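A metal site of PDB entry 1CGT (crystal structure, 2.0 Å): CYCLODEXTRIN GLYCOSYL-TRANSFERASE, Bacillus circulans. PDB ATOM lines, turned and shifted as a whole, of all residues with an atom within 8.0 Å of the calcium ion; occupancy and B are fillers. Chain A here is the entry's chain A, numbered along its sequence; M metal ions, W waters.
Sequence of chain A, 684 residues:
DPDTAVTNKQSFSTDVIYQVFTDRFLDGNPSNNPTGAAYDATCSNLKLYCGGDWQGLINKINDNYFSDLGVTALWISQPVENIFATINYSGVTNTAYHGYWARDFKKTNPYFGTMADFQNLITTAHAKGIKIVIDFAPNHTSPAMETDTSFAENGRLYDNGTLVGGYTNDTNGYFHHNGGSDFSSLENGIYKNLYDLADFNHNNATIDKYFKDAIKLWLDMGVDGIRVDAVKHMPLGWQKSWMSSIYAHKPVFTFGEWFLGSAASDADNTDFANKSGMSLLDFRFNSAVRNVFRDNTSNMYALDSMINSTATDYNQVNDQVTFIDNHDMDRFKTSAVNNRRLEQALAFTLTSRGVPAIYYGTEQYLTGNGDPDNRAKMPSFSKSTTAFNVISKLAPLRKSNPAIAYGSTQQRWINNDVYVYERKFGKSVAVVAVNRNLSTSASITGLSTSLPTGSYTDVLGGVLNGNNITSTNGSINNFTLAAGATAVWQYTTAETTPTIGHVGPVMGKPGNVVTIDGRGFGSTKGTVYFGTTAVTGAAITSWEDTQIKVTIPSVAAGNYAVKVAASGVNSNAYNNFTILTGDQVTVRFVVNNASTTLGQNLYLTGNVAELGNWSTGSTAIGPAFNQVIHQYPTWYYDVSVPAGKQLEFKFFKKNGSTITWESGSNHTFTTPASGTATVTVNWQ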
ATOM      1  N   THR A  22       9.424   5.214 -17.741  1.00  0.00           N
ATOM      2  CA  THR A  22       8.610   4.936 -16.563  1.00  0.00           C
ATOM      3  C   THR A  22       8.842   3.542 -15.978  1.00  0.00           C
ATOM      4  O   THR A  22       8.940   3.404 -14.759  1.00  0.00           O
ATOM      5  CB  THR A  22       7.130   5.077 -16.914  1.00  0.00           C
ATOM      6  OG1 THR A  22       7.002   6.360 -17.520  1.00  0.00           O
ATOM      7  CG2 THR A  22       6.204   4.974 -15.709  1.00  0.00           C
ATOM      8  N   ASP A  23       9.003   2.551 -16.845  1.00  0.00           N
ATOM      9  CA  ASP A  23       9.255   1.183 -16.432  1.00  0.00           C
ATOM     10  C   ASP A  23      10.562   0.951 -15.687  1.00  0.00           C
ATOM     11  O   ASP A  23      10.654   0.006 -14.878  1.00  0.00           O
ATOM     12  CB  ASP A  23       9.255   0.260 -17.647  1.00  0.00           C
ATOM     13  CG  ASP A  23       9.290  -1.197 -17.195  1.00  0.00           C
ATOM     14  OD1 ASP A  23       8.424  -1.608 -16.445  1.00  0.00           O
ATOM     15  OD2 ASP A  23      10.202  -1.904 -17.571  1.00  0.00           O
ATOM     16  N   LEU A  26      11.062   3.452 -10.902  1.00  0.00           N
ATOM     17  CA  LEU A  26      10.704   2.908  -9.598  1.00  0.00           C
ATOM     18  C   LEU A  26       9.349   2.198  -9.613  1.00  0.00           C
ATOM     19  O   LEU A  26       8.293   2.766  -9.929  1.00  0.00           O
ATOM     20  CB  LEU A  26      10.604   3.990  -8.535  1.00  0.00           C
ATOM     21  CG  LEU A  26      11.141   3.839  -7.092  1.00  0.00           C
ATOM     22  CD1 LEU A  26      10.211   4.643  -6.217  1.00  0.00           C
ATOM     23  CD2 LEU A  26      11.165   2.406  -6.589  1.00  0.00           C
ATOM     24  N   ASP A  27       9.342   0.925  -9.229  1.00  0.00           N
ATOM     25  CA  ASP A  27       8.120   0.176  -9.027  1.00  0.00           C
ATOM     26  C   ASP A  27       7.488   0.589  -7.712  1.00  0.00           C
ATOM     27  O   ASP A  27       7.729   0.019  -6.658  1.00  0.00           O
ATOM     28  CB  ASP A  27       8.453  -1.288  -9.047  1.00  0.00           C
ATOM     29  CG  ASP A  27       7.246  -2.208  -8.897  1.00  0.00           C
ATOM     30  OD1 ASP A  27       6.097  -1.780  -8.837  1.00  0.00           O
ATOM     31  OD2 ASP A  27       7.485  -3.392  -8.863  1.00  0.00           O
ATOM     32  N   GLY A  28       6.640   1.597  -7.763  1.00  0.00           N
ATOM     33  CA  GLY A  28       5.987   2.097  -6.584  1.00  0.00           C
ATOM     34  C   GLY A  28       4.758   1.287  -6.226  1.00  0.00           C
ATOM     35  O   GLY A  28       4.212   1.433  -5.135  1.00  0.00           O
ATOM     36  N   ASN A  29       4.287   0.422  -7.116  1.00  0.00           N
ATOM     37  CA  ASN A  29       3.095  -0.351  -6.846  1.00  0.00           C
ATOM     38  C   ASN A  29       3.237  -1.684  -7.520  1.00  0.00           C
ATOM     39  O   ASN A  29       2.970  -1.839  -8.713  1.00  0.00           O
ATOM     40  CB  ASN A  29       1.855   0.361  -7.368  1.00  0.00           C
ATOM     41  CG  ASN A  29       0.602  -0.499  -7.253  1.00  0.00           C
ATOM     42  OD1 ASN A  29      -0.411  -0.212  -7.881  1.00  0.00           O
ATOM     43  ND2 ASN A  29       0.546  -1.586  -6.483  1.00  0.00           N
ATOM     44  N   PRO A  30       3.755  -2.691  -6.816  1.00  0.00           N
ATOM     45  CA  PRO A  30       3.928  -4.040  -7.341  1.00  0.00           C
ATOM     46  C   PRO A  30       2.622  -4.697  -7.750  1.00  0.00           C
ATOM     47  O   PRO A  30       2.694  -5.568  -8.600  1.00  0.00           O
ATOM     48  CB  PRO A  30       4.624  -4.795  -6.237  1.00  0.00           C
ATOM     49  CG  PRO A  30       5.232  -3.683  -5.419  1.00  0.00           C
ATOM     50  CD  PRO A  30       4.119  -2.646  -5.401  1.00  0.00           C
ATOM     51  N   SER A  31       1.461  -4.300  -7.267  1.00  0.00           N
ATOM     52  CA  SER A  31       0.228  -4.981  -7.661  1.00  0.00           C
ATOM     53  C   SER A  31      -0.196  -4.762  -9.099  1.00  0.00           C
ATOM     54  O   SER A  31      -1.081  -5.474  -9.585  1.00  0.00           O
ATOM     55  CB  SER A  31      -0.943  -4.549  -6.835  1.00  0.00           C
ATOM     56  OG  SER A  31      -0.494  -4.022  -5.590  1.00  0.00           O
ATOM     57  N   ASN A  32       0.358  -3.735  -9.765  1.00  0.00           N
ATOM     58  CA  ASN A  32      -0.001  -3.500 -11.165  1.00  0.00           C
ATOM     59  C   ASN A  32       1.032  -4.114 -12.070  1.00  0.00           C
ATOM     60  O   ASN A  32       0.922  -3.949 -13.285  1.00  0.00           O
ATOM     61  CB  ASN A  32      -0.130  -1.984 -11.460  1.00  0.00           C
ATOM     62  CG  ASN A  32       1.077  -1.089 -11.232  1.00  0.00           C
ATOM     63  OD1 ASN A  32       2.268  -1.511 -11.181  1.00  0.00           O
ATOM     64  ND2 ASN A  32       0.780   0.176 -10.976  1.00  0.00           N
ATOM     65  N   ASN A  33       2.026  -4.848 -11.519  1.00  0.00           N
ATOM     66  CA  ASN A  33       3.071  -5.403 -12.358  1.00  0.00           C
ATOM     67  C   ASN A  33       2.537  -6.445 -13.305  1.00  0.00           C
ATOM     68  O   ASN A  33       1.499  -7.054 -13.000  1.00  0.00           O
ATOM     69  CB  ASN A  33       4.186  -6.050 -11.567  1.00  0.00           C
ATOM     70  CG  ASN A  33       5.038  -5.044 -10.804  1.00  0.00           C
ATOM     71  OD1 ASN A  33       4.827  -3.799 -10.787  1.00  0.00           O
ATOM     72  ND2 ASN A  33       6.006  -5.587 -10.086  1.00  0.00           N
ATOM     73  N   PRO A  34       3.123  -6.632 -14.490  1.00  0.00           N
ATOM     74  CA  PRO A  34       2.762  -7.718 -15.401  1.00  0.00           C
ATOM     75  C   PRO A  34       3.114  -9.051 -14.752  1.00  0.00           C
ATOM     76  O   PRO A  34       3.959  -9.147 -13.866  1.00  0.00           O
ATOM     77  CB  PRO A  34       3.574  -7.441 -16.667  1.00  0.00           C
ATOM     78  CG  PRO A  34       4.038  -6.016 -16.543  1.00  0.00           C
ATOM     79  CD  PRO A  34       4.233  -5.859 -15.051  1.00  0.00           C
ATOM     80  N   TYR A  39       7.322 -10.258 -17.238  1.00  0.00           N
ATOM     81  CA  TYR A  39       7.879  -9.488 -16.157  1.00  0.00           C
ATOM     82  C   TYR A  39       9.213  -9.999 -15.667  1.00  0.00           C
ATOM     83  O   TYR A  39       9.480 -11.193 -15.769  1.00  0.00           O
ATOM     84  CB  TYR A  39       6.838  -9.466 -15.066  1.00  0.00           C
ATOM     85  CG  TYR A  39       7.295  -8.830 -13.772  1.00  0.00           C
ATOM     86  CD1 TYR A  39       7.564  -7.474 -13.687  1.00  0.00           C
ATOM     87  CD2 TYR A  39       7.467  -9.643 -12.677  1.00  0.00           C
ATOM     88  CE1 TYR A  39       7.990  -6.934 -12.492  1.00  0.00           C
ATOM     89  CE2 TYR A  39       7.896  -9.118 -11.487  1.00  0.00           C
ATOM     90  CZ  TYR A  39       8.152  -7.764 -11.404  1.00  0.00           C
ATOM     91  OH  TYR A  39       8.570  -7.253 -10.181  1.00  0.00           O
ATOM     92  N   TYR A  49       9.334  -6.176 -18.856  1.00  0.00           N
ATOM     93  CA  TYR A  49       8.901  -5.193 -17.887  1.00  0.00           C
ATOM     94  C   TYR A  49       9.621  -5.413 -16.565  1.00  0.00           C
ATOM     95  O   TYR A  49       9.707  -6.500 -15.991  1.00  0.00           O
ATOM     96  CB  TYR A  49       7.421  -5.307 -17.645  1.00  0.00           C
ATOM     97  CG  TYR A  49       6.486  -4.631 -18.626  1.00  0.00           C
ATOM     98  CD1 TYR A  49       6.148  -3.334 -18.358  1.00  0.00           C
ATOM     99  CD2 TYR A  49       5.953  -5.295 -19.715  1.00  0.00           C
ATOM    100  CE1 TYR A  49       5.248  -2.659 -19.171  1.00  0.00           C
ATOM    101  CE2 TYR A  49       5.045  -4.647 -20.546  1.00  0.00           C
ATOM    102  CZ  TYR A  49       4.701  -3.317 -20.267  1.00  0.00           C
ATOM    103  OH  TYR A  49       3.806  -2.593 -21.061  1.00  0.00           O
ATOM    104  N   CYS A  50      10.143  -4.339 -16.021  1.00  0.00           N
ATOM    105  CA  CYS A  50      10.788  -4.342 -14.719  1.00  0.00           C
ATOM    106  C   CYS A  50       9.810  -3.876 -13.662  1.00  0.00           C
ATOM    107  O   CYS A  50      10.110  -3.972 -12.478  1.00  0.00           O
ATOM    108  CB  CYS A  50      12.018  -3.435 -14.819  1.00  0.00           C
ATOM    109  SG  CYS A  50      13.183  -4.211 -15.958  1.00  0.00           S
ATOM    110  N   GLY A  51       8.653  -3.324 -14.016  1.00  0.00           N
ATOM    111  CA  GLY A  51       7.641  -2.929 -13.057  1.00  0.00           C
ATOM    112  C   GLY A  51       7.547  -1.452 -12.649  1.00  0.00           C
ATOM    113  O   GLY A  51       6.664  -1.157 -11.801  1.00  0.00           O
ATOM    114  N   GLY A  52       8.405  -0.526 -13.139  1.00  0.00           N
ATOM    115  CA  GLY A  52       8.331   0.884 -12.757  1.00  0.00           C
ATOM    116  C   GLY A  52       7.026   1.518 -13.213  1.00  0.00           C
ATOM    117  O   GLY A  52       6.466   1.147 -14.268  1.00  0.00           O
ATOM    118  N   ASP A  53       6.505   2.467 -12.460  1.00  0.00           N
ATOM    119  CA  ASP A  53       5.162   2.959 -12.718  1.00  0.00           C
ATOM    120  C   ASP A  53       4.999   4.391 -12.233  1.00  0.00           C
ATOM    121  O   ASP A  53       5.942   4.975 -11.688  1.00  0.00           O
ATOM    122  CB  ASP A  53       4.151   1.990 -12.023  1.00  0.00           C
ATOM    123  CG  ASP A  53       4.427   1.691 -10.536  1.00  0.00           C
ATOM    124  OD1 ASP A  53       4.852   2.586  -9.810  1.00  0.00           O
ATOM    125  OD2 ASP A  53       4.224   0.550 -10.114  1.00  0.00           O
ATOM    126  N   TRP A  54       3.794   4.946 -12.354  1.00  0.00           N
ATOM    127  CA  TRP A  54       3.538   6.308 -11.964  1.00  0.00           C
ATOM    128  C   TRP A  54       3.517   6.461 -10.467  1.00  0.00           C
ATOM    129  O   TRP A  54       3.929   7.517  -9.998  1.00  0.00           O
ATOM    130  CB  TRP A  54       2.209   6.823 -12.552  1.00  0.00           C
ATOM    131  CG  TRP A  54       2.168   6.867 -14.096  1.00  0.00           C
ATOM    132  CD1 TRP A  54       3.294   7.072 -14.870  1.00  0.00           C
ATOM    133  CD2 TRP A  54       1.054   6.654 -14.888  1.00  0.00           C
ATOM    134  NE1 TRP A  54       2.910   6.956 -16.126  1.00  0.00           N
ATOM    135  CE2 TRP A  54       1.588   6.719 -16.184  1.00  0.00           C
ATOM    136  CE3 TRP A  54      -0.304   6.424 -14.695  1.00  0.00           C
ATOM    137  CZ2 TRP A  54       0.802   6.537 -17.291  1.00  0.00           C
ATOM    138  CZ3 TRP A  54      -1.090   6.250 -15.809  1.00  0.00           C
ATOM    139  CH2 TRP A  54      -0.550   6.303 -17.085  1.00  0.00           C
ATOM    140  N   GLN A  55       3.141   5.458  -9.654  1.00  0.00           N
ATOM    141  CA  GLN A  55       3.278   5.586  -8.182  1.00  0.00           C
ATOM    142  C   GLN A  55       4.755   5.746  -7.824  1.00  0.00           C
ATOM    143  O   GLN A  55       5.094   6.512  -6.930  1.00  0.00           O
ATOM    144  CB  GLN A  55       2.735   4.327  -7.430  1.00  0.00           C
ATOM    145  CG  GLN A  55       2.757   4.453  -5.904  1.00  0.00           C
ATOM    146  CD  GLN A  55       1.968   5.679  -5.443  1.00  0.00           C
ATOM    147  OE1 GLN A  55       0.795   5.870  -5.820  1.00  0.00           O
ATOM    148  NE2 GLN A  55       2.549   6.590  -4.666  1.00  0.00           N
ATOM    149  N   GLY A  56       5.659   5.088  -8.543  1.00  0.00           N
ATOM    150  CA  GLY A  56       7.090   5.196  -8.273  1.00  0.00           C
ATOM    151  C   GLY A  56       7.590   6.615  -8.505  1.00  0.00           C
ATOM    152  O   GLY A  56       8.409   7.120  -7.722  1.00  0.00           O
ATOM    153  N   PRO A 110      -2.146   0.042 -18.053  1.00  0.00           N
ATOM    154  CA  PRO A 110      -2.451  -0.422 -16.689  1.00  0.00           C
ATOM    155  C   PRO A 110      -1.223  -0.779 -15.892  1.00  0.00           C
ATOM    156  O   PRO A 110      -1.262  -0.753 -14.661  1.00  0.00           O
ATOM    157  CB  PRO A 110      -3.406  -1.576 -16.897  1.00  0.00           C
ATOM    158  CG  PRO A 110      -2.895  -2.202 -18.178  1.00  0.00           C
ATOM    159  CD  PRO A 110      -2.670  -0.942 -19.021  1.00  0.00           C
ATOM    160  N   TYR A 111      -0.110  -1.114 -16.544  1.00  0.00           N
ATOM    161  CA  TYR A 111       1.119  -1.381 -15.828  1.00  0.00           C
ATOM    162  C   TYR A 111       1.741  -0.126 -15.293  1.00  0.00           C
ATOM    163  O   TYR A 111       2.490  -0.188 -14.320  1.00  0.00           O
ATOM    164  CB  TYR A 111       2.086  -2.069 -16.714  1.00  0.00           C
ATOM    165  CG  TYR A 111       1.479  -3.347 -17.230  1.00  0.00           C
ATOM    166  CD1 TYR A 111       0.792  -4.217 -16.372  1.00  0.00           C
ATOM    167  CD2 TYR A 111       1.613  -3.659 -18.572  1.00  0.00           C
ATOM    168  CE1 TYR A 111       0.240  -5.397 -16.856  1.00  0.00           C
ATOM    169  CE2 TYR A 111       1.075  -4.837 -19.055  1.00  0.00           C
ATOM    170  CZ  TYR A 111       0.388  -5.706 -18.196  1.00  0.00           C
ATOM    171  OH  TYR A 111      -0.092  -6.915 -18.706  1.00  0.00           O
ATOM    172  N   PHE A 112       1.448   1.055 -15.865  1.00  0.00           N
ATOM    173  CA  PHE A 112       1.967   2.273 -15.274  1.00  0.00           C
ATOM    174  C   PHE A 112       0.928   2.808 -14.306  1.00  0.00           C
ATOM    175  O   PHE A 112       1.306   3.469 -13.338  1.00  0.00           O
ATOM    176  CB  PHE A 112       2.269   3.339 -16.341  1.00  0.00           C
ATOM    177  CG  PHE A 112       3.261   2.977 -17.442  1.00  0.00           C
ATOM    178  CD1 PHE A 112       4.317   2.108 -17.204  1.00  0.00           C
ATOM    179  CD2 PHE A 112       3.135   3.560 -18.708  1.00  0.00           C
ATOM    180  CE1 PHE A 112       5.221   1.830 -18.218  1.00  0.00           C
ATOM    181  CE2 PHE A 112       4.053   3.276 -19.714  1.00  0.00           C
ATOM    182  CZ  PHE A 112       5.100   2.410 -19.471  1.00  0.00           C
ATOM    183  N   GLY A 113      -0.379   2.630 -14.525  1.00  0.00           N
ATOM    184  CA  GLY A 113      -1.366   3.053 -13.562  1.00  0.00           C
ATOM    185  C   GLY A 113      -2.742   3.245 -14.189  1.00  0.00           C
ATOM    186  O   GLY A 113      -2.936   3.046 -15.396  1.00  0.00           O
HETATM  187 CA    CA M   1       4.461  -1.656 -10.830  1.00  0.00          CA
HETATM  188  O   HOH W   1       4.260  -1.778 -13.033  1.00  0.00           O
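OD1 of Asp 53 lies within hydrogen-bond range of N of Gln 55, at 3.3 Å.
OD1 of Asp 53 lies within hydrogen-bond range of N of Gly 56 (2.9 Å).
The side-chain hydroxyl (OH) of Tyr 39 lies within hydrogen-bond range of the side-chain amide nitrogen (ND2) of Asn 33 (3.1 Å).
O of Thr 22 is in hydrogen-bond range of N of Asp 53 (3.5 Å).
The backbone NH (N) of Asp 53 sits at hydrogen-bond distance from the backbone carbonyl oxygen (O) of Leu 26 (3.1 Å).
OD1 of Asn 32 lies close to O of Tyr 111 (3.4 Å).
The side-chain carboxylate (OD1) of Asp 53 sits at hydrogen-bond distance from the backbone NH (N) of Gly 28 (2.9 Å).
The side-chain amide nitrogen (ND2) of Asn 29 sits at hydrogen-bond distance from the side-chain hydroxyl (OG) of Ser 31, at 2.8 Å.
Of the 24 residues printed, 6 come within 4 Å of the calcium ion.
The nearest printed residue that does not touch the calcium ion is Pro 30 (4.2 Å).
The calcium ion is bound by the side-chain amide oxygen of Asn 33, water W1, the side-chain amide oxygen of Asn 32, the side-chain carboxylate of Asp 53, the backbone carbonyl oxygen of Gly 51, the side-chain carboxylate of Asp 27 and the backbone carbonyl oxygen of Asn 29.
The calcium ion has seven donor atoms within binding distance.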
